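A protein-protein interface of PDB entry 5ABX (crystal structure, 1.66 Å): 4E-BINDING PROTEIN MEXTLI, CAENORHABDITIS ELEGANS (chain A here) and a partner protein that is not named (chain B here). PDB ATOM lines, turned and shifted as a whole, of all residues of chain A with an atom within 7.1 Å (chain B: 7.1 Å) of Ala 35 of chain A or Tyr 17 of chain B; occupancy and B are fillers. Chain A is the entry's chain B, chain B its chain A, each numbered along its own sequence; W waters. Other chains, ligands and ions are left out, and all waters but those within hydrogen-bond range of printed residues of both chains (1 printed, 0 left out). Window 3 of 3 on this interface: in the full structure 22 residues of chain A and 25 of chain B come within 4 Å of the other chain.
CB of Glu 30 of chain A touches O of Val 33 of chain B, 3.5 Å away. Ile 31 of chain A touches Val 33 of chain B. Met 32 of chain B touches Val 34 of chain A. Val 34 of chain A touches Val 33 of chain B (CG2 to CA, 3.7 Å). Tyr 17 of chain B touches Ala 35 of chain A. Asp 37 of chain A touches Lys 19 of chain B. Tyr 17 of chain B touches Ile 38 of chain A. Ile 38 of chain A touches Ile 49 of chain B. Ile 38 of chain A touches Tyr 61 of chain B.
Printed residues of chain B within 4 Å of Ile 31 of chain A: Val 33 (3.8 Å). Of the printed residues of chain B, Asp 37 of chain A touches Tyr 17 and Lys 19. Of the printed residues of chain B, Ile 38 of chain A touches Tyr 17 (3.6 Å), Ile 49 (3.2 Å) and Tyr 61 (3.7 Å). Of chain A, only Ala 35 (3.7 Å), Asp 37 (2.6 Å) and Ile 38 (3.6 Å) come within 4 Å of Tyr 17 of chain B. Leu 30 of chain B touches none of the printed residues of chain A. Lys 31 of chain B touches none of the printed residues of chain A. Of the printed residues of chain A, Met 32 of chain B touches Val 34. Of the printed residues of chain A, Ile 49 of chain B touches Ile 38. The nearest residue of chain B that does not touch Ala 35 of chain A is Val 33 of chain B (4.03 Å). The nearest printed residue of chain A that does not touch Tyr 17 of chain B is Val 34 of chain A (5.3 Å). The nearest printed residue of chain A that does not touch Met 32 of chain B is Glu 30 of chain A (6.0 Å).
Of the 19 printed residues of chain B, 6 touch a printed residue of chain A. Hydrophobic or aromatic side chains of chain B that line the printed part of chain A: Tyr 17, Val 33, Ile 49 and Tyr 61. Hydrophobic or aromatic side chains of chain A within 4 Å of the printed part of chain B: Ile 31, Val 34, Ala 35 and Ile 38. Among the printed residues, 10 pairs touch across the chains. Among the printed residues, no Asp or Glu carboxylate lies within 4 Å of a Lys or Arg side-chain nitrogen of the other chain.
The backbone carbonyl oxygen of Lys 31 of chain B sits at hydrogen-bond distance from the backbone NH of Tyr 17 of chain B, at 2.9 Å. The backbone carbonyl oxygen of Lys 19 of chain B lies close to the side-chain sulfur of Cys 29 of chain B, 3.7 Å away. N of Val 33 of chain B lies within hydrogen-bond range of O of Leu 15 of chain B (2.7 Å).
OH of Tyr 17 of chain B is in hydrogen-bond range of OD2 of Asp 37 of chain A, at 2.6 Å.
Water W1 lies within hydrogen-bond range of O of Val 34 of chain A and NZ of Lys 19 of chain B.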
ATOM      1  N   GLN A  29      29.674   2.175  26.997  1.00  0.00           N
ATOM      2  CA  GLN A  29      29.220   3.455  27.547  1.00  0.00           C
ATOM      3  C   GLN A  29      28.497   4.278  26.492  1.00  0.00           C
ATOM      4  O   GLN A  29      27.424   4.835  26.736  1.00  0.00           O
ATOM      5  CB  GLN A  29      30.393   4.270  28.084  1.00  0.00           C
ATOM      6  CG  GLN A  29      31.073   3.705  29.321  1.00  0.00           C
ATOM      7  CD  GLN A  29      32.377   4.419  29.614  1.00  0.00           C
ATOM      8  OE1 GLN A  29      32.534   5.587  29.271  1.00  0.00           O
ATOM      9  NE2 GLN A  29      33.329   3.715  30.222  1.00  0.00           N
ATOM     10  N   GLU A  30      29.096   4.334  25.309  1.00  0.00           N
ATOM     11  CA  GLU A  30      28.575   5.169  24.235  1.00  0.00           C
ATOM     12  C   GLU A  30      27.239   4.647  23.744  1.00  0.00           C
ATOM     13  O   GLU A  30      26.294   5.421  23.578  1.00  0.00           O
ATOM     14  CB  GLU A  30      29.587   5.246  23.084  1.00  0.00           C
ATOM     15  CG  GLU A  30      30.828   6.068  23.430  1.00  0.00           C
ATOM     16  CD  GLU A  30      32.007   5.837  22.487  1.00  0.00           C
ATOM     17  OE1 GLU A  30      31.882   5.048  21.525  1.00  0.00           O
ATOM     18  OE2 GLU A  30      33.073   6.448  22.722  1.00  0.00           O
ATOM     19  N   ILE A  31      27.137   3.340  23.531  1.00  0.00           N
ATOM     20  CA  ILE A  31      25.895   2.772  23.020  1.00  0.00           C
ATOM     21  C   ILE A  31      24.791   2.934  24.058  1.00  0.00           C
ATOM     22  O   ILE A  31      23.681   3.324  23.731  1.00  0.00           O
ATOM     23  CB  ILE A  31      26.040   1.290  22.662  1.00  0.00           C
ATOM     24  CG1 ILE A  31      27.120   1.096  21.601  1.00  0.00           C
ATOM     25  CG2 ILE A  31      24.713   0.733  22.127  1.00  0.00           C
ATOM     26  CD1 ILE A  31      27.542  -0.338  21.431  1.00  0.00           C
ATOM     27  N   ASN A  32      25.098   2.655  25.322  1.00  0.00           N
ATOM     28  CA  ASN A  32      24.081   2.755  26.351  1.00  0.00           C
ATOM     29  C   ASN A  32      23.599   4.191  26.524  1.00  0.00           C
ATOM     30  O   ASN A  32      22.415   4.428  26.763  1.00  0.00           O
ATOM     31  CB  ASN A  32      24.604   2.214  27.688  1.00  0.00           C
ATOM     32  CG  ASN A  32      23.500   2.035  28.698  1.00  0.00           C
ATOM     33  OD1 ASN A  32      22.532   1.322  28.447  1.00  0.00           O
ATOM     34  ND2 ASN A  32      23.641   2.675  29.856  1.00  0.00           N
ATOM     35  N   ARG A  33      24.507   5.150  26.380  1.00  0.00           N
ATOM     36  CA  ARG A  33      24.158   6.547  26.590  1.00  0.00           C
ATOM     37  C   ARG A  33      23.262   7.117  25.482  1.00  0.00           C
ATOM     38  O   ARG A  33      22.349   7.885  25.780  1.00  0.00           O
ATOM     39  CB  ARG A  33      25.416   7.411  26.711  1.00  0.00           C
ATOM     40  CG  ARG A  33      25.129   8.830  27.195  1.00  0.00           C
ATOM     41  CD  ARG A  33      26.353   9.732  27.097  1.00  0.00           C
ATOM     42  NE  ARG A  33      27.598   8.990  27.287  1.00  0.00           N
ATOM     43  CZ  ARG A  33      28.462   8.677  26.322  1.00  0.00           C
ATOM     44  NH1 ARG A  33      28.251   9.044  25.060  1.00  0.00           N
ATOM     45  NH2 ARG A  33      29.558   7.993  26.626  1.00  0.00           N
ATOM     46  N   VAL A  34      23.507   6.762  24.218  1.00  0.00           N
ATOM     47  CA  VAL A  34      22.782   7.401  23.116  1.00  0.00           C
ATOM     48  C   VAL A  34      21.779   6.474  22.429  1.00  0.00           C
ATOM     49  O   VAL A  34      20.811   6.944  21.836  1.00  0.00           O
ATOM     50  CB  VAL A  34      23.744   7.969  22.031  1.00  0.00           C
ATOM     51  CG1 VAL A  34      24.746   8.952  22.647  1.00  0.00           C
ATOM     52  CG2 VAL A  34      24.459   6.876  21.293  1.00  0.00           C
ATOM     53  N   ALA A  35      22.007   5.167  22.500  1.00  0.00           N
ATOM     54  CA  ALA A  35      21.104   4.208  21.859  1.00  0.00           C
ATOM     55  C   ALA A  35      20.918   2.949  22.693  1.00  0.00           C
ATOM     56  O   ALA A  35      21.190   1.838  22.227  1.00  0.00           O
ATOM     57  CB  ALA A  35      21.627   3.844  20.462  1.00  0.00           C
ATOM     58  N   PRO A  36      20.415   3.109  23.924  1.00  0.00           N
ATOM     59  CA  PRO A  36      20.300   1.978  24.850  1.00  0.00           C
ATOM     60  C   PRO A  36      19.474   0.832  24.291  1.00  0.00           C
ATOM     61  O   PRO A  36      19.733  -0.328  24.611  1.00  0.00           O
ATOM     62  CB  PRO A  36      19.612   2.594  26.075  1.00  0.00           C
ATOM     63  CG  PRO A  36      18.969   3.853  25.571  1.00  0.00           C
ATOM     64  CD  PRO A  36      19.868   4.349  24.494  1.00  0.00           C
ATOM     65  N   ASP A  37      18.500   1.154  23.451  1.00  0.00           N
ATOM     66  CA  ASP A  37      17.589   0.139  22.959  1.00  0.00           C
ATOM     67  C   ASP A  37      18.215  -0.855  21.959  1.00  0.00           C
ATOM     68  O   ASP A  37      17.663  -1.939  21.757  1.00  0.00           O
ATOM     69  CB  ASP A  37      16.349   0.811  22.343  1.00  0.00           C
ATOM     70  CG  ASP A  37      16.692   1.967  21.405  1.00  0.00           C
ATOM     71  OD1 ASP A  37      17.558   2.816  21.744  1.00  0.00           O
ATOM     72  OD2 ASP A  37      16.063   2.035  20.329  1.00  0.00           O
ATOM     73  N   ILE A  38      19.355  -0.522  21.350  1.00  0.00           N
ATOM     74  CA  ILE A  38      19.976  -1.448  20.394  1.00  0.00           C
ATOM     75  C   ILE A  38      21.037  -2.335  21.058  1.00  0.00           C
ATOM     76  O   ILE A  38      21.501  -3.295  20.460  1.00  0.00           O
ATOM     77  CB  ILE A  38      20.606  -0.702  19.180  1.00  0.00           C
ATOM     78  CG1 ILE A  38      21.937  -0.026  19.549  1.00  0.00           C
ATOM     79  CG2 ILE A  38      19.591   0.282  18.595  1.00  0.00           C
ATOM     80  CD1 ILE A  38      22.658   0.617  18.369  1.00  0.00           C
ATOM     81  N   LEU A  39      21.398  -2.028  22.300  1.00  0.00           N
ATOM     82  CA  LEU A  39      22.496  -2.735  22.959  1.00  0.00           C
ATOM     83  C   LEU A  39      22.115  -4.173  23.308  1.00  0.00           C
ATOM     84  O   LEU A  39      21.037  -4.434  23.845  1.00  0.00           O
ATOM     85  CB  LEU A  39      22.932  -1.977  24.221  1.00  0.00           C
ATOM     86  CG  LEU A  39      24.132  -2.563  24.973  1.00  0.00           C
ATOM     87  CD1 LEU A  39      25.393  -2.513  24.118  1.00  0.00           C
ATOM     88  CD2 LEU A  39      24.331  -1.833  26.311  1.00  0.00           C
ATOM     89  N   LEU B  15      29.023   4.508  13.355  1.00  0.00           N
ATOM     90  CA  LEU B  15      27.662   3.985  13.303  1.00  0.00           C
ATOM     91  C   LEU B  15      26.695   5.035  13.814  1.00  0.00           C
ATOM     92  O   LEU B  15      26.852   5.542  14.926  1.00  0.00           O
ATOM     93  CB  LEU B  15      27.521   2.708  14.138  1.00  0.00           C
ATOM     94  CG  LEU B  15      26.113   2.101  14.183  1.00  0.00           C
ATOM     95  CD1 LEU B  15      25.748   1.509  12.834  1.00  0.00           C
ATOM     96  CD2 LEU B  15      26.002   1.062  15.285  1.00  0.00           C
ATOM     97  N   TRP B  16      25.698   5.354  12.994  1.00  0.00           N
ATOM     98  CA  TRP B  16      24.589   6.207  13.415  1.00  0.00           C
ATOM     99  C   TRP B  16      23.312   5.369  13.467  1.00  0.00           C
ATOM    100  O   TRP B  16      23.170   4.379  12.754  1.00  0.00           O
ATOM    101  CB  TRP B  16      24.376   7.398  12.476  1.00  0.00           C
ATOM    102  CG  TRP B  16      25.572   8.298  12.220  1.00  0.00           C
ATOM    103  CD1 TRP B  16      26.755   7.964  11.623  1.00  0.00           C
ATOM    104  CD2 TRP B  16      25.661   9.702  12.524  1.00  0.00           C
ATOM    105  NE1 TRP B  16      27.589   9.072  11.561  1.00  0.00           N
ATOM    106  CE2 TRP B  16      26.931  10.147  12.100  1.00  0.00           C
ATOM    107  CE3 TRP B  16      24.785  10.622  13.113  1.00  0.00           C
ATOM    108  CZ2 TRP B  16      27.345  11.472  12.250  1.00  0.00           C
ATOM    109  CZ3 TRP B  16      25.201  11.933  13.260  1.00  0.00           C
ATOM    110  CH2 TRP B  16      26.470  12.344  12.834  1.00  0.00           C
ATOM    111  N   TYR B  17      22.400   5.785  14.335  1.00  0.00           N
ATOM    112  CA  TYR B  17      21.138   5.099  14.546  1.00  0.00           C
ATOM    113  C   TYR B  17      20.026   6.137  14.506  1.00  0.00           C
ATOM    114  O   TYR B  17      20.153   7.219  15.079  1.00  0.00           O
ATOM    115  CB  TYR B  17      21.173   4.349  15.882  1.00  0.00           C
ATOM    116  CG  TYR B  17      19.851   3.813  16.366  1.00  0.00           C
ATOM    117  CD1 TYR B  17      19.131   2.906  15.608  1.00  0.00           C
ATOM    118  CD2 TYR B  17      19.341   4.192  17.596  1.00  0.00           C
ATOM    119  CE1 TYR B  17      17.914   2.403  16.056  1.00  0.00           C
ATOM    120  CE2 TYR B  17      18.142   3.689  18.057  1.00  0.00           C
ATOM    121  CZ  TYR B  17      17.434   2.793  17.280  1.00  0.00           C
ATOM    122  OH  TYR B  17      16.230   2.287  17.728  1.00  0.00           O
ATOM    123  N   LEU B  18      18.957   5.815  13.789  1.00  0.00           N
ATOM    124  CA  LEU B  18      17.777   6.664  13.742  1.00  0.00           C
ATOM    125  C   LEU B  18      16.602   5.870  14.264  1.00  0.00           C
ATOM    126  O   LEU B  18      16.279   4.819  13.725  1.00  0.00           O
ATOM    127  CB  LEU B  18      17.514   7.161  12.324  1.00  0.00           C
ATOM    128  CG  LEU B  18      16.404   8.219  12.223  1.00  0.00           C
ATOM    129  CD1 LEU B  18      16.680   9.135  11.050  1.00  0.00           C
ATOM    130  CD2 LEU B  18      15.021   7.590  12.089  1.00  0.00           C
ATOM    131  N   LYS B  19      15.994   6.367  15.339  1.00  0.00           N
ATOM    132  CA  LYS B  19      14.782   5.782  15.889  1.00  0.00           C
ATOM    133  C   LYS B  19      13.625   6.688  15.526  1.00  0.00           C
ATOM    134  O   LYS B  19      13.649   7.879  15.833  1.00  0.00           O
ATOM    135  CB  LYS B  19      14.879   5.622  17.409  1.00  0.00           C
ATOM    136  CG  LYS B  19      13.644   4.984  18.039  1.00  0.00           C
ATOM    137  CD  LYS B  19      13.837   4.680  19.523  1.00  0.00           C
ATOM    138  CE  LYS B  19      14.189   5.923  20.326  1.00  0.00           C
ATOM    139  NZ  LYS B  19      15.663   6.130  20.427  1.00  0.00           N
ATOM    140  N   ALA B  20      12.628   6.125  14.855  1.00  0.00           N
ATOM    141  CA  ALA B  20      11.464   6.897  14.446  1.00  0.00           C
ATOM    142  C   ALA B  20      10.817   7.577  15.648  1.00  0.00           C
ATOM    143  O   ALA B  20      10.684   6.985  16.717  1.00  0.00           O
ATOM    144  CB  ALA B  20      10.463   6.008  13.736  1.00  0.00           C
ATOM    145  N   CYS B  29      16.146  12.837  14.940  1.00  0.00           N
ATOM    146  CA  CYS B  29      16.029  11.421  15.287  1.00  0.00           C
ATOM    147  C   CYS B  29      17.363  10.694  15.153  1.00  0.00           C
ATOM    148  O   CYS B  29      17.507   9.548  15.578  1.00  0.00           O
ATOM    149  CB  CYS B  29      15.008  10.734  14.387  1.00  0.00           C
ATOM    150  SG  CYS B  29      13.307  11.312  14.635  1.00  0.00           S
ATOM    151  N   LEU B  30      18.322  11.377  14.545  1.00  0.00           N
ATOM    152  CA  LEU B  30      19.594  10.787  14.151  1.00  0.00           C
ATOM    153  C   LEU B  30      20.639  10.986  15.239  1.00  0.00           C
ATOM    154  O   LEU B  30      20.819  12.100  15.734  1.00  0.00           O
ATOM    155  CB  LEU B  30      20.027  11.429  12.830  1.00  0.00           C
ATOM    156  CG  LEU B  30      21.282  10.978  12.112  1.00  0.00           C
ATOM    157  CD1 LEU B  30      21.130   9.559  11.618  1.00  0.00           C
ATOM    158  CD2 LEU B  30      21.522  11.942  10.963  1.00  0.00           C
ATOM    159  N   LYS B  31      21.306   9.902  15.629  1.00  0.00           N
ATOM    160  CA  LYS B  31      22.323   9.957  16.673  1.00  0.00           C
ATOM    161  C   LYS B  31      23.555   9.176  16.244  1.00  0.00           C
ATOM    162  O   LYS B  31      23.446   8.050  15.748  1.00  0.00           O
ATOM    163  CB  LYS B  31      21.786   9.389  17.986  1.00  0.00           C
ATOM    164  CG  LYS B  31      20.442   9.966  18.431  1.00  0.00           C
ATOM    165  CD  LYS B  31      20.542  11.433  18.854  1.00  0.00           C
ATOM    166  CE  LYS B  31      21.346  11.596  20.126  1.00  0.00           C
ATOM    167  NZ  LYS B  31      21.089  12.907  20.778  1.00  0.00           N
ATOM    168  N   MET B  32      24.721   9.774  16.454  1.00  0.00           N
ATOM    169  CA  MET B  32      25.981   9.078  16.255  1.00  0.00           C
ATOM    170  C   MET B  32      26.272   8.212  17.477  1.00  0.00           C
ATOM    171  O   MET B  32      26.387   8.713  18.603  1.00  0.00           O
ATOM    172  CB  MET B  32      27.112  10.078  16.008  1.00  0.00           C
ATOM    173  CG  MET B  32      28.299   9.496  15.275  1.00  0.00           C
ATOM    174  SD  MET B  32      29.289   8.335  16.237  1.00  0.00           S
ATOM    175  CE  MET B  32      29.871   9.364  17.583  1.00  0.00           C
ATOM    176  N   VAL B  33      26.391   6.909  17.249  1.00  0.00           N
ATOM    177  CA  VAL B  33      26.485   5.947  18.333  1.00  0.00           C
ATOM    178  C   VAL B  33      27.938   5.681  18.732  1.00  0.00           C
ATOM    179  O   VAL B  33      28.322   5.916  19.877  1.00  0.00           O
ATOM    180  CB  VAL B  33      25.792   4.627  17.956  1.00  0.00           C
ATOM    181  CG1 VAL B  33      25.905   3.623  19.069  1.00  0.00           C
ATOM    182  CG2 VAL B  33      24.314   4.875  17.646  1.00  0.00           C
ATOM    183  N   ILE B  49      25.019  -5.267  18.950  1.00  0.00           N
ATOM    184  CA  ILE B  49      23.882  -4.392  18.686  1.00  0.00           C
ATOM    185  C   ILE B  49      22.822  -5.177  17.921  1.00  0.00           C
ATOM    186  O   ILE B  49      23.117  -6.204  17.311  1.00  0.00           O
ATOM    187  CB  ILE B  49      24.254  -3.112  17.897  1.00  0.00           C
ATOM    188  CG1 ILE B  49      24.814  -3.457  16.514  1.00  0.00           C
ATOM    189  CG2 ILE B  49      25.218  -2.243  18.719  1.00  0.00           C
ATOM    190  CD1 ILE B  49      25.179  -2.249  15.681  1.00  0.00           C
ATOM    191  N   LEU B  55      15.424  -4.552  14.102  1.00  0.00           N
ATOM    192  CA  LEU B  55      15.047  -3.172  14.395  1.00  0.00           C
ATOM    193  C   LEU B  55      13.554  -2.957  14.202  1.00  0.00           C
ATOM    194  O   LEU B  55      12.933  -3.581  13.346  1.00  0.00           O
ATOM    195  CB  LEU B  55      15.813  -2.191  13.505  1.00  0.00           C
ATOM    196  CG  LEU B  55      17.311  -2.026  13.768  1.00  0.00           C
ATOM    197  CD1 LEU B  55      17.888  -1.094  12.731  1.00  0.00           C
ATOM    198  CD2 LEU B  55      17.568  -1.491  15.168  1.00  0.00           C
ATOM    199  N   ASN B  56      12.992  -2.048  14.988  1.00  0.00           N
ATOM    200  CA  ASN B  56      11.594  -1.679  14.840  1.00  0.00           C
ATOM    201  C   ASN B  56      11.365  -0.944  13.520  1.00  0.00           C
ATOM    202  O   ASN B  56      12.289  -0.359  12.958  1.00  0.00           O
ATOM    203  CB  ASN B  56      11.152  -0.815  16.022  1.00  0.00           C
ATOM    204  CG  ASN B  56       9.795  -1.215  16.560  1.00  0.00           C
ATOM    205  OD1 ASN B  56       8.855  -1.462  15.801  1.00  0.00           O
ATOM    206  ND2 ASN B  56       9.687  -1.291  17.880  1.00  0.00           N
ATOM    207  N   SER B  59      13.044   2.544  11.815  1.00  0.00           N
ATOM    208  CA  SER B  59      14.411   2.752  12.310  1.00  0.00           C
ATOM    209  C   SER B  59      15.436   2.523  11.207  1.00  0.00           C
ATOM    210  O   SER B  59      15.179   1.765  10.270  1.00  0.00           O
ATOM    211  CB  SER B  59      14.718   1.821  13.485  1.00  0.00           C
ATOM    212  OG  SER B  59      14.005   2.208  14.648  1.00  0.00           O
ATOM    213  N   ASP B  60      16.596   3.176  11.350  1.00  0.00           N
ATOM    214  CA  ASP B  60      17.712   3.084  10.398  1.00  0.00           C
ATOM    215  C   ASP B  60      19.042   2.825  11.105  1.00  0.00           C
ATOM    216  O   ASP B  60      19.255   3.265  12.238  1.00  0.00           O
ATOM    217  CB  ASP B  60      17.927   4.381   9.606  1.00  0.00           C
ATOM    218  CG  ASP B  60      16.668   4.946   8.978  1.00  0.00           C
ATOM    219  OD1 ASP B  60      15.794   4.184   8.516  1.00  0.00           O
ATOM    220  OD2 ASP B  60      16.595   6.194   8.895  1.00  0.00           O
ATOM    221  N   TYR B  61      19.962   2.181  10.398  1.00  0.00           N
ATOM    222  CA  TYR B  61      21.382   2.287  10.727  1.00  0.00           C
ATOM    223  C   TYR B  61      22.107   2.997   9.586  1.00  0.00           C
ATOM    224  O   TYR B  61      21.750   2.824   8.417  1.00  0.00           O
ATOM    225  CB  TYR B  61      22.029   0.926  10.925  1.00  0.00           C
ATOM    226  CG  TYR B  61      21.780   0.196  12.216  1.00  0.00           C
ATOM    227  CD1 TYR B  61      21.861   0.836  13.451  1.00  0.00           C
ATOM    228  CD2 TYR B  61      21.541  -1.166  12.203  1.00  0.00           C
ATOM    229  CE1 TYR B  61      21.673   0.127  14.632  1.00  0.00           C
ATOM    230  CE2 TYR B  61      21.355  -1.875  13.367  1.00  0.00           C
ATOM    231  CZ  TYR B  61      21.417  -1.228  14.580  1.00  0.00           C
ATOM    232  OH  TYR B  61      21.240  -1.951  15.736  1.00  0.00           O
ATOM    233  N   TYR B  62      23.137   3.767   9.932  1.00  0.00           N
ATOM    234  CA  TYR B  62      24.029   4.392   8.953  1.00  0.00           C
ATOM    235  C   TYR B  62      25.455   4.058   9.354  1.00  0.00           C
ATOM    236  O   TYR B  62      25.795   4.156  10.535  1.00  0.00           O
ATOM    237  CB  TYR B  62      23.859   5.915   8.898  1.00  0.00           C
ATOM    238  CG  TYR B  62      22.455   6.407   8.644  1.00  0.00           C
ATOM    239  CD1 TYR B  62      21.493   6.404   9.650  1.00  0.00           C
ATOM    240  CD2 TYR B  62      22.099   6.894   7.397  1.00  0.00           C
ATOM    241  CE1 TYR B  62      20.207   6.864   9.400  1.00  0.00           C
ATOM    242  CE2 TYR B  62      20.826   7.358   7.150  1.00  0.00           C
ATOM    243  CZ  TYR B  62      19.890   7.340   8.148  1.00  0.00           C
ATOM    244  OH  TYR B  62      18.621   7.801   7.868  1.00  0.00           O
ATOM    245  N   PRO B  70      25.505  11.564   7.834  1.00  0.00           N
ATOM    246  CA  PRO B  70      24.660  10.819   6.896  1.00  0.00           C
ATOM    247  C   PRO B  70      23.425  11.619   6.480  1.00  0.00           C
ATOM    248  O   PRO B  70      22.281  11.233   6.739  1.00  0.00           O
ATOM    249  CB  PRO B  70      24.294   9.560   7.685  1.00  0.00           C
ATOM    250  CG  PRO B  70      24.294  10.001   9.096  1.00  0.00           C
ATOM    251  CD  PRO B  70      25.364  11.060   9.213  1.00  0.00           C
HETATM  252  O   HOH W   1      18.745   6.629  20.202  1.00  0.00           O
